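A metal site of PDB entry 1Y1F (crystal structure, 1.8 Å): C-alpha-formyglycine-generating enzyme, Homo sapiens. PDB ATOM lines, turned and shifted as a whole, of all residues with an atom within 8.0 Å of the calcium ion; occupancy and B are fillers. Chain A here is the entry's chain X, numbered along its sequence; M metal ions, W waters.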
ATOM      1  N   HIS A 184      -3.652 -14.580   0.323  1.00  0.00           N
ATOM      2  CA  HIS A 184      -3.054 -14.745  -0.996  1.00  0.00           C
ATOM      3  C   HIS A 184      -2.830 -13.376  -1.644  1.00  0.00           C
ATOM      4  O   HIS A 184      -3.743 -12.552  -1.663  1.00  0.00           O
ATOM      5  CB  HIS A 184      -3.904 -15.653  -1.888  1.00  0.00           C
ATOM      6  CG  HIS A 184      -3.792 -17.086  -1.531  1.00  0.00           C
ATOM      7  ND1 HIS A 184      -2.694 -17.840  -1.867  1.00  0.00           N
ATOM      8  CD2 HIS A 184      -4.607 -17.897  -0.805  1.00  0.00           C
ATOM      9  CE1 HIS A 184      -2.823 -19.055  -1.345  1.00  0.00           C
ATOM     10  NE2 HIS A 184      -3.987 -19.125  -0.724  1.00  0.00           N
ATOM     11  N   ALA A 186      -1.095 -13.156  -4.861  1.00  0.00           N
ATOM     12  CA  ALA A 186      -0.870 -13.352  -6.305  1.00  0.00           C
ATOM     13  C   ALA A 186      -1.527 -14.641  -6.744  1.00  0.00           C
ATOM     14  O   ALA A 186      -1.773 -15.556  -5.942  1.00  0.00           O
ATOM     15  CB  ALA A 186       0.611 -13.391  -6.605  1.00  0.00           C
ATOM     16  N   ASN A 187      -1.812 -14.709  -8.045  1.00  0.00           N
ATOM     17  CA  ASN A 187      -2.393 -15.868  -8.650  1.00  0.00           C
ATOM     18  C   ASN A 187      -1.287 -16.802  -9.185  1.00  0.00           C
ATOM     19  O   ASN A 187      -0.737 -16.595 -10.271  1.00  0.00           O
ATOM     20  CB  ASN A 187      -3.383 -15.468  -9.728  1.00  0.00           C
ATOM     21  CG  ASN A 187      -3.989 -16.675 -10.433  1.00  0.00           C
ATOM     22  OD1 ASN A 187      -4.082 -17.752  -9.848  1.00  0.00           O
ATOM     23  ND2 ASN A 187      -4.432 -16.497 -11.691  1.00  0.00           N
ATOM     24  N   ILE A 188      -0.947 -17.817  -8.378  1.00  0.00           N
ATOM     25  CA  ILE A 188      -0.044 -18.900  -8.760  1.00  0.00           C
ATOM     26  C   ILE A 188      -0.768 -20.262  -8.567  1.00  0.00           C
ATOM     27  O   ILE A 188      -1.995 -20.292  -8.543  1.00  0.00           O
ATOM     28  CB  ILE A 188       1.301 -18.769  -8.058  1.00  0.00           C
ATOM     29  CG1 ILE A 188       1.139 -18.811  -6.513  1.00  0.00           C
ATOM     30  CG2 ILE A 188       1.931 -17.475  -8.464  1.00  0.00           C
ATOM     31  CD1 ILE A 188       2.437 -19.005  -5.763  1.00  0.00           C
ATOM     32  N   TRP A 189      -0.025 -21.350  -8.468  1.00  0.00           N
ATOM     33  CA  TRP A 189      -0.579 -22.679  -8.350  1.00  0.00           C
ATOM     34  C   TRP A 189      -0.572 -23.132  -6.875  1.00  0.00           C
ATOM     35  O   TRP A 189       0.407 -22.894  -6.183  1.00  0.00           O
ATOM     36  CB  TRP A 189       0.287 -23.620  -9.172  1.00  0.00           C
ATOM     37  CG  TRP A 189      -0.186 -25.053  -9.278  1.00  0.00           C
ATOM     38  CD1 TRP A 189      -0.088 -26.038  -8.320  1.00  0.00           C
ATOM     39  CD2 TRP A 189      -0.740 -25.663 -10.430  1.00  0.00           C
ATOM     40  NE1 TRP A 189      -0.608 -27.232  -8.817  1.00  0.00           N
ATOM     41  CE2 TRP A 189      -1.017 -27.027 -10.107  1.00  0.00           C
ATOM     42  CE3 TRP A 189      -1.086 -25.197 -11.712  1.00  0.00           C
ATOM     43  CZ2 TRP A 189      -1.583 -27.913 -11.018  1.00  0.00           C
ATOM     44  CZ3 TRP A 189      -1.635 -26.093 -12.624  1.00  0.00           C
ATOM     45  CH2 TRP A 189      -1.871 -27.428 -12.280  1.00  0.00           C
ATOM     46  N   GLN A 190      -1.652 -23.749  -6.420  1.00  0.00           N
ATOM     47  CA  GLN A 190      -1.642 -24.492  -5.166  1.00  0.00           C
ATOM     48  C   GLN A 190      -2.004 -25.934  -5.477  1.00  0.00           C
ATOM     49  O   GLN A 190      -2.852 -26.175  -6.319  1.00  0.00           O
ATOM     50  CB  GLN A 190      -2.616 -23.957  -4.126  1.00  0.00           C
ATOM     51  CG  GLN A 190      -2.276 -22.544  -3.648  1.00  0.00           C
ATOM     52  CD  GLN A 190      -2.820 -21.513  -4.618  1.00  0.00           C
ATOM     53  OE1 GLN A 190      -3.964 -21.653  -5.102  1.00  0.00           O
ATOM     54  NE2 GLN A 190      -2.052 -20.458  -4.867  1.00  0.00           N
ATOM     55  N   ASN A 197      -4.588 -28.568  -9.392  1.00  0.00           N
ATOM     56  CA  ASN A 197      -4.579 -27.167  -8.957  1.00  0.00           C
ATOM     57  C   ASN A 197      -5.823 -26.947  -8.088  1.00  0.00           C
ATOM     58  O   ASN A 197      -6.986 -27.021  -8.554  1.00  0.00           O
ATOM     59  CB  ASN A 197      -4.556 -26.224 -10.182  1.00  0.00           C
ATOM     60  CG  ASN A 197      -4.398 -24.772  -9.796  1.00  0.00           C
ATOM     61  OD1 ASN A 197      -4.597 -24.391  -8.630  1.00  0.00           O
ATOM     62  ND2 ASN A 197      -4.087 -23.934 -10.773  1.00  0.00           N
ATOM     63  N   THR A 198      -5.589 -26.762  -6.798  1.00  0.00           N
ATOM     64  CA  THR A 198      -6.714 -26.691  -5.872  1.00  0.00           C
ATOM     65  C   THR A 198      -7.567 -25.438  -6.022  1.00  0.00           C
ATOM     66  O   THR A 198      -8.684 -25.399  -5.523  1.00  0.00           O
ATOM     67  CB  THR A 198      -6.248 -26.784  -4.400  1.00  0.00           C
ATOM     68  OG1 THR A 198      -5.425 -25.673  -4.076  1.00  0.00           O
ATOM     69  CG2 THR A 198      -5.465 -27.998  -4.137  1.00  0.00           C
ATOM     70  N   GLY A 199      -7.024 -24.385  -6.672  1.00  0.00           N
ATOM     71  CA  GLY A 199      -7.702 -23.095  -6.769  1.00  0.00           C
ATOM     72  C   GLY A 199      -7.915 -22.438  -5.429  1.00  0.00           C
ATOM     73  O   GLY A 199      -8.847 -21.660  -5.275  1.00  0.00           O
ATOM     74  N   GLU A 200      -7.035 -22.724  -4.470  1.00  0.00           N
ATOM     75  CA  GLU A 200      -7.088 -22.105  -3.152  1.00  0.00           C
ATOM     76  C   GLU A 200      -7.060 -20.578  -3.201  1.00  0.00           C
ATOM     77  O   GLU A 200      -7.815 -19.927  -2.427  1.00  0.00           O
ATOM     78  CB  GLU A 200      -5.947 -22.629  -2.290  1.00  0.00           C
ATOM     79  CG  GLU A 200      -5.922 -22.119  -0.853  1.00  0.00           C
ATOM     80  CD  GLU A 200      -4.565 -22.375  -0.202  1.00  0.00           C
ATOM     81  OE1 GLU A 200      -3.928 -23.414  -0.503  1.00  0.00           O
ATOM     82  OE2 GLU A 200      -4.144 -21.526   0.606  1.00  0.00           O
ATOM     83  N   ASP A 201      -6.294 -20.003  -4.146  1.00  0.00           N
ATOM     84  CA  ASP A 201      -6.142 -18.538  -4.227  1.00  0.00           C
ATOM     85  C   ASP A 201      -7.335 -17.866  -4.934  1.00  0.00           C
ATOM     86  O   ASP A 201      -7.388 -16.641  -5.056  1.00  0.00           O
ATOM     87  CB  ASP A 201      -4.808 -18.138  -4.835  1.00  0.00           C
ATOM     88  CG  ASP A 201      -4.669 -18.578  -6.262  1.00  0.00           C
ATOM     89  OD1 ASP A 201      -5.695 -18.912  -6.911  1.00  0.00           O
ATOM     90  OD2 ASP A 201      -3.526 -18.616  -6.739  1.00  0.00           O
ATOM     91  N   GLY A 202      -8.320 -18.667  -5.364  1.00  0.00           N
ATOM     92  CA  GLY A 202      -9.540 -18.167  -5.977  1.00  0.00           C
ATOM     93  C   GLY A 202      -9.598 -18.344  -7.494  1.00  0.00           C
ATOM     94  O   GLY A 202     -10.639 -18.102  -8.110  1.00  0.00           O
ATOM     95  N   PHE A 203      -8.480 -18.783  -8.091  1.00  0.00           N
ATOM     96  CA  PHE A 203      -8.350 -18.919  -9.554  1.00  0.00           C
ATOM     97  C   PHE A 203      -7.467 -20.072  -9.978  1.00  0.00           C
ATOM     98  O   PHE A 203      -6.306 -20.159  -9.570  1.00  0.00           O
ATOM     99  CB  PHE A 203      -7.800 -17.630 -10.165  1.00  0.00           C
ATOM    100  CG  PHE A 203      -8.586 -16.441  -9.766  1.00  0.00           C
ATOM    101  CD1 PHE A 203      -9.739 -16.096 -10.463  1.00  0.00           C
ATOM    102  CD2 PHE A 203      -8.211 -15.695  -8.637  1.00  0.00           C
ATOM    103  CE1 PHE A 203     -10.506 -14.999 -10.069  1.00  0.00           C
ATOM    104  CE2 PHE A 203      -8.999 -14.616  -8.229  1.00  0.00           C
ATOM    105  CZ  PHE A 203     -10.141 -14.264  -8.965  1.00  0.00           C
ATOM    106  N   GLN A 204      -8.025 -20.962 -10.785  1.00  0.00           N
ATOM    107  CA  GLN A 204      -7.281 -22.066 -11.370  1.00  0.00           C
ATOM    108  C   GLN A 204      -6.490 -21.604 -12.597  1.00  0.00           C
ATOM    109  O   GLN A 204      -5.278 -21.895 -12.717  1.00  0.00           O
ATOM    110  CB  GLN A 204      -8.209 -23.221 -11.703  1.00  0.00           C
ATOM    111  CG  GLN A 204      -8.523 -24.036 -10.426  1.00  0.00           C
ATOM    112  CD  GLN A 204      -9.600 -25.031 -10.616  1.00  0.00           C
ATOM    113  OE1 GLN A 204     -10.587 -24.761 -11.304  1.00  0.00           O
ATOM    114  NE2 GLN A 204      -9.469 -26.211  -9.964  1.00  0.00           N
ATOM    115  N   GLY A 205      -7.171 -20.883 -13.479  1.00  0.00           N
ATOM    116  CA  GLY A 205      -6.608 -20.281 -14.657  1.00  0.00           C
ATOM    117  C   GLY A 205      -6.228 -18.860 -14.279  1.00  0.00           C
ATOM    118  O   GLY A 205      -5.844 -18.598 -13.156  1.00  0.00           O
ATOM    119  N   THR A 206      -6.334 -17.934 -15.223  1.00  0.00           N
ATOM    120  CA  THR A 206      -6.100 -16.551 -14.947  1.00  0.00           C
ATOM    121  C   THR A 206      -7.193 -15.952 -14.073  1.00  0.00           C
ATOM    122  O   THR A 206      -8.300 -16.528 -13.879  1.00  0.00           O
ATOM    123  CB  THR A 206      -6.052 -15.731 -16.280  1.00  0.00           C
ATOM    124  OG1 THR A 206      -7.282 -15.903 -16.987  1.00  0.00           O
ATOM    125  CG2 THR A 206      -4.930 -16.197 -17.135  1.00  0.00           C
ATOM    126  N   ALA A 207      -6.845 -14.810 -13.517  1.00  0.00           N
ATOM    127  CA  ALA A 207      -7.716 -13.949 -12.771  1.00  0.00           C
ATOM    128  C   ALA A 207      -7.931 -12.632 -13.512  1.00  0.00           C
ATOM    129  O   ALA A 207      -7.125 -12.250 -14.376  1.00  0.00           O
ATOM    130  CB  ALA A 207      -7.106 -13.679 -11.382  1.00  0.00           C
ATOM    131  N   PHE A 212      -6.349  -9.194  -6.694  1.00  0.00           N
ATOM    132  CA  PHE A 212      -5.273  -9.234  -5.692  1.00  0.00           C
ATOM    133  C   PHE A 212      -4.795  -7.822  -5.310  1.00  0.00           C
ATOM    134  O   PHE A 212      -5.120  -6.844  -5.991  1.00  0.00           O
ATOM    135  CB  PHE A 212      -4.132 -10.182  -6.135  1.00  0.00           C
ATOM    136  CG  PHE A 212      -4.579 -11.614  -6.218  1.00  0.00           C
ATOM    137  CD1 PHE A 212      -4.782 -12.354  -5.038  1.00  0.00           C
ATOM    138  CD2 PHE A 212      -4.932 -12.184  -7.409  1.00  0.00           C
ATOM    139  CE1 PHE A 212      -5.263 -13.625  -5.076  1.00  0.00           C
ATOM    140  CE2 PHE A 212      -5.400 -13.470  -7.461  1.00  0.00           C
ATOM    141  CZ  PHE A 212      -5.587 -14.181  -6.282  1.00  0.00           C
ATOM    142  N   ASN A 225      -0.337 -14.678 -12.345  1.00  0.00           N
ATOM    143  CA  ASN A 225      -1.387 -14.484 -13.352  1.00  0.00           C
ATOM    144  C   ASN A 225      -0.826 -14.790 -14.725  1.00  0.00           C
ATOM    145  O   ASN A 225      -0.599 -15.953 -15.024  1.00  0.00           O
ATOM    146  CB  ASN A 225      -2.062 -13.108 -13.205  1.00  0.00           C
ATOM    147  CG  ASN A 225      -3.561 -13.151 -13.535  1.00  0.00           C
ATOM    148  OD1 ASN A 225      -4.229 -14.175 -13.375  1.00  0.00           O
ATOM    149  ND2 ASN A 225      -4.098 -12.003 -13.959  1.00  0.00           N
ATOM    150  N   SER A 261       3.491 -16.961 -13.505  1.00  0.00           N
ATOM    151  CA  SER A 261       2.130 -17.126 -13.967  1.00  0.00           C
ATOM    152  C   SER A 261       1.300 -17.928 -12.989  1.00  0.00           C
ATOM    153  O   SER A 261       1.821 -18.457 -12.007  1.00  0.00           O
ATOM    154  CB  SER A 261       2.110 -17.805 -15.338  1.00  0.00           C
ATOM    155  OG  SER A 261       2.221 -19.229 -15.261  1.00  0.00           O
ATOM    156  N   TYR A 262       0.002 -18.047 -13.298  1.00  0.00           N
ATOM    157  CA  TYR A 262      -0.890 -18.939 -12.559  1.00  0.00           C
ATOM    158  C   TYR A 262      -0.454 -20.398 -12.473  1.00  0.00           C
ATOM    159  O   TYR A 262      -0.992 -21.142 -11.638  1.00  0.00           O
ATOM    160  CB  TYR A 262      -2.311 -18.878 -13.125  1.00  0.00           C
ATOM    161  CG  TYR A 262      -2.499 -19.445 -14.505  1.00  0.00           C
ATOM    162  CD1 TYR A 262      -2.441 -18.625 -15.638  1.00  0.00           C
ATOM    163  CD2 TYR A 262      -2.757 -20.786 -14.686  1.00  0.00           C
ATOM    164  CE1 TYR A 262      -2.640 -19.164 -16.936  1.00  0.00           C
ATOM    165  CE2 TYR A 262      -2.936 -21.335 -15.954  1.00  0.00           C
ATOM    166  CZ  TYR A 262      -2.888 -20.513 -17.077  1.00  0.00           C
ATOM    167  OH  TYR A 262      -3.103 -21.070 -18.329  1.00  0.00           O
ATOM    168  N   MET A 263       0.483 -20.809 -13.312  1.00  0.00           N
ATOM    169  CA  MET A 263       1.007 -22.178 -13.289  1.00  0.00           C
ATOM    170  C   MET A 263       2.113 -22.430 -12.317  1.00  0.00           C
ATOM    171  O   MET A 263       2.432 -23.594 -12.046  1.00  0.00           O
ATOM    172  CB  MET A 263       1.587 -22.537 -14.645  1.00  0.00           C
ATOM    173  CG  MET A 263       0.521 -22.678 -15.699  1.00  0.00           C
ATOM    174  SD  MET A 263       1.096 -23.031 -17.357  1.00  0.00           S
ATOM    175  CE  MET A 263       1.896 -24.626 -17.133  1.00  0.00           C
ATOM    176  N   CSO A 264       2.718 -21.379 -11.794  1.00  0.00           N
ATOM    177  CA  CSO A 264       3.946 -21.538 -11.027  1.00  0.00           C
ATOM    178  CB  CSO A 264       4.705 -20.224 -10.950  1.00  0.00           C
ATOM    179  SG  CSO A 264       6.412 -20.538 -10.484  1.00  0.00           S
ATOM    180  C   CSO A 264       3.681 -22.099  -9.621  1.00  0.00           C
ATOM    181  O   CSO A 264       2.794 -21.632  -8.929  1.00  0.00           O
HETATM  182 CA    CA M   1      -4.237 -19.797  -8.727  1.00  0.00          CA
HETATM  183  O   HOH W   1      -3.573 -21.024 -10.772  1.00  0.00           O
HETATM  184  O   HOH W   2      -4.605 -21.893  -7.623  1.00  0.00           O
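The calcium ion is bound by O of Phe 203, at 2.3 Å.
The calcium ion is bound by O of Ile 188 (2.3 Å).
The side-chain amide oxygen (OD1) of Asn 187 binds the calcium ion (2.3 Å).
The calcium ion is bound by water W2, at 2.4 Å.
OD2 of Asp 201 binds the calcium ion, 2.4 Å away.
Water W1 binds the calcium ion (2.5 Å).
OD1 of Asp 201 binds the calcium ion.
Water W2 lies within hydrogen-bond range of the side-chain amide oxygen (OE1) of Gln 190 (2.6 Å) and the side-chain amide oxygen (OD1) of Asn 197 (2.7 Å).
Water W1 lies within hydrogen-bond range of O of Tyr 262, O of Gln 204 and ND2 of Asn 197.
Four residues have an atom within 4 Å of the calcium ion: Asn 187, Ile 188, Asp 201 and Phe 203.
The backbone carbonyl oxygen (O) of Asn 187 sits close to the backbone NH (N) of Tyr 262.
The side-chain amide nitrogen of Asn 187 is in hydrogen-bond range of the backbone carbonyl oxygen of Gly 205, 2.9 Å away.
ND2 of Asn 187 sits close to N of Ala 207 (3.5 Å).
N of Asn 225 is in hydrogen-bond range of O of Asn 187, 2.9 Å away.
The side-chain amide oxygen (OE1) of Gln 190 sits at hydrogen-bond distance from the backbone NH (N) of Asp 201 (3.0 Å).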
